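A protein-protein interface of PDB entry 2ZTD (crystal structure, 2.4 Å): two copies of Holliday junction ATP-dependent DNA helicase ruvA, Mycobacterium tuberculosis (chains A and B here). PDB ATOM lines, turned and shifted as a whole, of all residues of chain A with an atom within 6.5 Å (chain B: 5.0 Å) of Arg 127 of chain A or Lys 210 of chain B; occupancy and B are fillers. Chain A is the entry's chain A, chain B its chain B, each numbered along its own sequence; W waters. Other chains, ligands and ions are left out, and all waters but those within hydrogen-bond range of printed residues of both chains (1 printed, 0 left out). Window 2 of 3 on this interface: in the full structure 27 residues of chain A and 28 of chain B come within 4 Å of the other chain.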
ATOM      1  N   VAL A 107      16.102 -21.100   1.370  1.00  0.00           N
ATOM      2  CA  VAL A 107      16.311 -19.855   0.611  1.00  0.00           C
ATOM      3  C   VAL A 107      16.514 -20.118  -0.876  1.00  0.00           C
ATOM      4  O   VAL A 107      15.924 -19.445  -1.709  1.00  0.00           O
ATOM      5  CB  VAL A 107      17.500 -19.014   1.152  1.00  0.00           C
ATOM      6  CG1 VAL A 107      17.877 -17.923   0.157  1.00  0.00           C
ATOM      7  CG2 VAL A 107      17.153 -18.404   2.506  1.00  0.00           C
ATOM      8  N   HIS A 108      17.356 -21.094  -1.200  1.00  0.00           N
ATOM      9  CA  HIS A 108      17.526 -21.543  -2.582  1.00  0.00           C
ATOM     10  C   HIS A 108      17.130 -23.007  -2.737  1.00  0.00           C
ATOM     11  O   HIS A 108      17.761 -23.900  -2.159  1.00  0.00           O
ATOM     12  CB  HIS A 108      18.980 -21.397  -3.046  1.00  0.00           C
ATOM     13  CG  HIS A 108      19.539 -20.020  -2.893  1.00  0.00           C
ATOM     14  ND1 HIS A 108      18.984 -18.923  -3.513  1.00  0.00           N
ATOM     15  CD2 HIS A 108      20.598 -19.558  -2.187  1.00  0.00           C
ATOM     16  CE1 HIS A 108      19.678 -17.840  -3.201  1.00  0.00           C
ATOM     17  NE2 HIS A 108      20.661 -18.201  -2.394  1.00  0.00           N
ATOM     18  N   ASN A 121      28.469 -18.529  -7.204  1.00  0.00           N
ATOM     19  CA  ASN A 121      27.767 -17.283  -6.916  1.00  0.00           C
ATOM     20  C   ASN A 121      27.741 -17.021  -5.413  1.00  0.00           C
ATOM     21  O   ASN A 121      26.810 -17.425  -4.711  1.00  0.00           O
ATOM     22  CB  ASN A 121      26.361 -17.290  -7.521  1.00  0.00           C
ATOM     23  CG  ASN A 121      25.661 -15.949  -7.382  1.00  0.00           C
ATOM     24  OD1 ASN A 121      26.036 -15.115  -6.550  1.00  0.00           O
ATOM     25  ND2 ASN A 121      24.626 -15.737  -8.188  1.00  0.00           N
ATOM     26  N   VAL A 122      28.786 -16.356  -4.934  1.00  0.00           N
ATOM     27  CA  VAL A 122      28.966 -16.071  -3.517  1.00  0.00           C
ATOM     28  C   VAL A 122      27.938 -15.063  -2.991  1.00  0.00           C
ATOM     29  O   VAL A 122      27.543 -15.124  -1.818  1.00  0.00           O
ATOM     30  CB  VAL A 122      30.400 -15.549  -3.245  1.00  0.00           C
ATOM     31  CG1 VAL A 122      30.532 -15.050  -1.817  1.00  0.00           C
ATOM     32  CG2 VAL A 122      31.421 -16.627  -3.541  1.00  0.00           C
ATOM     33  N   ALA A 123      27.510 -14.149  -3.858  1.00  0.00           N
ATOM     34  CA  ALA A 123      26.525 -13.136  -3.474  1.00  0.00           C
ATOM     35  C   ALA A 123      25.188 -13.796  -3.174  1.00  0.00           C
ATOM     36  O   ALA A 123      24.539 -13.499  -2.164  1.00  0.00           O
ATOM     37  CB  ALA A 123      26.368 -12.121  -4.564  1.00  0.00           C
ATOM     38  N   ALA A 124      24.789 -14.699  -4.066  1.00  0.00           N
ATOM     39  CA  ALA A 124      23.603 -15.510  -3.864  1.00  0.00           C
ATOM     40  C   ALA A 124      23.732 -16.241  -2.549  1.00  0.00           C
ATOM     41  O   ALA A 124      22.834 -16.188  -1.711  1.00  0.00           O
ATOM     42  CB  ALA A 124      23.453 -16.501  -4.992  1.00  0.00           C
ATOM     43  N   LEU A 125      24.866 -16.919  -2.378  1.00  0.00           N
ATOM     44  CA  LEU A 125      25.120 -17.738  -1.202  1.00  0.00           C
ATOM     45  C   LEU A 125      25.057 -16.938   0.083  1.00  0.00           C
ATOM     46  O   LEU A 125      24.542 -17.412   1.096  1.00  0.00           O
ATOM     47  CB  LEU A 125      26.483 -18.407  -1.306  1.00  0.00           C
ATOM     48  CG  LEU A 125      26.519 -19.833  -1.849  1.00  0.00           C
ATOM     49  CD1 LEU A 125      27.961 -20.322  -1.997  1.00  0.00           C
ATOM     50  CD2 LEU A 125      25.724 -20.777  -0.950  1.00  0.00           C
ATOM     51  N   THR A 126      25.589 -15.722   0.041  1.00  0.00           N
ATOM     52  CA  THR A 126      25.665 -14.897   1.236  1.00  0.00           C
ATOM     53  C   THR A 126      24.279 -14.398   1.645  1.00  0.00           C
ATOM     54  O   THR A 126      24.069 -13.976   2.784  1.00  0.00           O
ATOM     55  CB  THR A 126      26.658 -13.746   1.050  1.00  0.00           C
ATOM     56  OG1 THR A 126      27.964 -14.286   0.820  1.00  0.00           O
ATOM     57  CG2 THR A 126      26.699 -12.863   2.285  1.00  0.00           C
ATOM     58  N   ARG A 127      23.326 -14.474   0.716  1.00  0.00           N
ATOM     59  CA  ARG A 127      21.944 -14.125   1.016  1.00  0.00           C
ATOM     60  C   ARG A 127      21.353 -15.051   2.093  1.00  0.00           C
ATOM     61  O   ARG A 127      20.290 -14.768   2.642  1.00  0.00           O
ATOM     62  CB  ARG A 127      21.094 -14.131  -0.262  1.00  0.00           C
ATOM     63  CG  ARG A 127      21.368 -12.926  -1.189  1.00  0.00           C
ATOM     64  CD  ARG A 127      20.824 -13.118  -2.604  1.00  0.00           C
ATOM     65  NE  ARG A 127      21.662 -12.459  -3.607  1.00  0.00           N
ATOM     66  CZ  ARG A 127      21.666 -12.750  -4.907  1.00  0.00           C
ATOM     67  NH1 ARG A 127      20.867 -13.706  -5.378  1.00  0.00           N
ATOM     68  NH2 ARG A 127      22.469 -12.083  -5.738  1.00  0.00           N
ATOM     69  N   VAL A 128      22.051 -16.139   2.400  1.00  0.00           N
ATOM     70  CA  VAL A 128      21.600 -17.084   3.426  1.00  0.00           C
ATOM     71  C   VAL A 128      22.047 -16.674   4.839  1.00  0.00           C
ATOM     72  O   VAL A 128      23.249 -16.537   5.087  1.00  0.00           O
ATOM     73  CB  VAL A 128      22.122 -18.522   3.130  1.00  0.00           C
ATOM     74  CG1 VAL A 128      21.767 -19.473   4.260  1.00  0.00           C
ATOM     75  CG2 VAL A 128      21.568 -19.036   1.810  1.00  0.00           C
ATOM     76  N   PRO A 129      21.091 -16.495   5.775  1.00  0.00           N
ATOM     77  CA  PRO A 129      21.529 -16.158   7.136  1.00  0.00           C
ATOM     78  C   PRO A 129      22.537 -17.197   7.615  1.00  0.00           C
ATOM     79  O   PRO A 129      22.300 -18.395   7.488  1.00  0.00           O
ATOM     80  CB  PRO A 129      20.238 -16.241   7.962  1.00  0.00           C
ATOM     81  CG  PRO A 129      19.135 -16.070   6.983  1.00  0.00           C
ATOM     82  CD  PRO A 129      19.631 -16.665   5.685  1.00  0.00           C
ATOM     83  N   ILE A 131      25.626 -17.614   6.464  1.00  0.00           N
ATOM     84  CA  ILE A 131      26.690 -17.813   5.481  1.00  0.00           C
ATOM     85  C   ILE A 131      27.377 -16.502   5.104  1.00  0.00           C
ATOM     86  O   ILE A 131      26.840 -15.704   4.322  1.00  0.00           O
ATOM     87  CB  ILE A 131      26.167 -18.491   4.209  1.00  0.00           C
ATOM     88  CG1 ILE A 131      25.392 -19.766   4.559  1.00  0.00           C
ATOM     89  CG2 ILE A 131      27.304 -18.793   3.263  1.00  0.00           C
ATOM     90  CD1 ILE A 131      25.006 -20.563   3.340  1.00  0.00           C
ATOM     91  N   PHE B 176      17.095 -15.387   9.526  1.00  0.00           N
ATOM     92  CA  PHE B 176      16.855 -14.008   9.117  1.00  0.00           C
ATOM     93  C   PHE B 176      16.609 -13.093  10.317  1.00  0.00           C
ATOM     94  O   PHE B 176      16.121 -13.533  11.360  1.00  0.00           O
ATOM     95  CB  PHE B 176      15.701 -13.914   8.110  1.00  0.00           C
ATOM     96  CG  PHE B 176      16.027 -14.478   6.752  1.00  0.00           C
ATOM     97  CD1 PHE B 176      16.761 -13.743   5.833  1.00  0.00           C
ATOM     98  CD2 PHE B 176      15.606 -15.759   6.400  1.00  0.00           C
ATOM     99  CE1 PHE B 176      17.077 -14.284   4.585  1.00  0.00           C
ATOM    100  CE2 PHE B 176      15.904 -16.289   5.155  1.00  0.00           C
ATOM    101  CZ  PHE B 176      16.643 -15.555   4.243  1.00  0.00           C
ATOM    102  N   SER B 206      11.533 -16.392  -1.385  1.00  0.00           N
ATOM    103  CA  SER B 206      11.914 -16.174  -2.778  1.00  0.00           C
ATOM    104  C   SER B 206      12.497 -14.779  -3.020  1.00  0.00           C
ATOM    105  O   SER B 206      13.506 -14.632  -3.701  1.00  0.00           O
ATOM    106  CB  SER B 206      10.707 -16.405  -3.677  1.00  0.00           C
ATOM    107  OG  SER B 206      10.987 -15.994  -4.989  1.00  0.00           O
ATOM    108  N   LEU B 207      11.852 -13.758  -2.459  1.00  0.00           N
ATOM    109  CA  LEU B 207      12.368 -12.402  -2.493  1.00  0.00           C
ATOM    110  C   LEU B 207      13.704 -12.315  -1.767  1.00  0.00           C
ATOM    111  O   LEU B 207      14.634 -11.685  -2.251  1.00  0.00           O
ATOM    112  CB  LEU B 207      11.383 -11.431  -1.826  1.00  0.00           C
ATOM    113  CG  LEU B 207      10.038 -11.183  -2.507  1.00  0.00           C
ATOM    114  CD1 LEU B 207       9.221 -10.131  -1.746  1.00  0.00           C
ATOM    115  CD2 LEU B 207      10.265 -10.729  -3.937  1.00  0.00           C
ATOM    116  N   LEU B 208      13.785 -12.912  -0.588  1.00  0.00           N
ATOM    117  CA  LEU B 208      15.007 -12.838   0.205  1.00  0.00           C
ATOM    118  C   LEU B 208      16.188 -13.543  -0.473  1.00  0.00           C
ATOM    119  O   LEU B 208      17.349 -13.263  -0.162  1.00  0.00           O
ATOM    120  CB  LEU B 208      14.761 -13.397   1.601  1.00  0.00           C
ATOM    121  CG  LEU B 208      13.813 -12.611   2.500  1.00  0.00           C
ATOM    122  CD1 LEU B 208      13.334 -13.479   3.658  1.00  0.00           C
ATOM    123  CD2 LEU B 208      14.515 -11.365   3.007  1.00  0.00           C
ATOM    124  N   GLY B 209      15.890 -14.469  -1.387  1.00  0.00           N
ATOM    125  CA  GLY B 209      16.912 -15.187  -2.131  1.00  0.00           C
ATOM    126  C   GLY B 209      17.434 -14.284  -3.225  1.00  0.00           C
ATOM    127  O   GLY B 209      18.398 -14.602  -3.924  1.00  0.00           O
ATOM    128  N   LYS B 210      16.769 -13.151  -3.337  1.00  0.00           N
ATOM    129  CA  LYS B 210      17.215 -11.955  -4.034  1.00  0.00           C
ATOM    130  C   LYS B 210      17.656 -11.945  -5.468  1.00  0.00           C
ATOM    131  O   LYS B 210      16.868 -12.153  -6.371  1.00  0.00           O
ATOM    132  CB  LYS B 210      18.271 -11.228  -3.195  1.00  0.00           C
ATOM    133  CG  LYS B 210      17.687 -10.346  -2.102  1.00  0.00           C
ATOM    134  CD  LYS B 210      18.768  -9.688  -1.273  1.00  0.00           C
ATOM    135  CE  LYS B 210      19.021 -10.442   0.020  1.00  0.00           C
ATOM    136  NZ  LYS B 210      20.370 -10.147   0.591  1.00  0.00           N
HETATM  137  O   HOH W   1      15.217 -17.277  -3.359  1.00  0.00           O
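The guanidinium group (NH1) of Arg 127 of chain A is in hydrogen-bond range of the backbone carbonyl oxygen (O) of Gly 209 of chain B.
O of Ala 123 of chain A sits close to NE of Arg 127 of chain A. NE2 of His 108 of chain A lies within hydrogen-bond range of O of Ala 124 of chain A, at 3.0 Å.
Phe 176 of chain B touches Val 107 of chain A (CZ to CG2, 3.4 Å). Gly 209 of chain B touches Val 107 of chain A. His 108 of chain A touches Gly 209 of chain B (CE1 to O, 3.6 Å). Phe 176 of chain B touches Arg 127 of chain A. Leu 208 of chain B touches Arg 127 of chain A. Lys 210 of chain B touches Arg 127 of chain A. N of Phe 176 of chain B touches CG of Pro 129 of chain A (3.3 Å).
Of the printed residues of chain B, Val 107 of chain A touches Phe 176 and Gly 209. Thr 126 of chain A touches none of the printed residues of chain B. Of the printed residues of chain B, Arg 127 of chain A touches Phe 176 (3.8 Å), Leu 208 (3.8 Å), Gly 209 (3.0 Å) and Lys 210 (3.2 Å). Val 128 of chain A touches none of the printed residues of chain B. Of the printed residues of chain B, Pro 129 of chain A touches Phe 176 (3.3 Å). Lys 210 of chain B touches just one residue of chain A: Arg 127. The nearest residue of chain A that does not touch Lys 210 of chain B is His 108 of chain A (5.5 Å).
Of the 12 printed residues of chain A, 4 touch a printed residue of chain B. Hydrophobic or aromatic side chains of chain A within 4 Å of the printed part of chain B: Val 107, His 108 and Pro 129. Along chain A the printed residues that touch a printed residue of chain B span positions 107 to 129. Of the 6 printed residues of chain B, 4 touch a printed residue of chain A. Hydrophobic or aromatic side chains of chain B that line the printed part of chain A: Phe 176. Among the printed residues, 8 pairs touch across the chains. Among the printed residues, no Asp or Glu carboxylate lies within 4 Å of a Lys or Arg side-chain nitrogen of the other chain.
No position is printed for both chains.
Water W1 lies within hydrogen-bond range of the backbone carbonyl oxygen (O) of Val 107 of chain A, the backbone carbonyl oxygen (O) of Ser 206 of chain B and the backbone NH (N) of Gly 209 of chain B.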
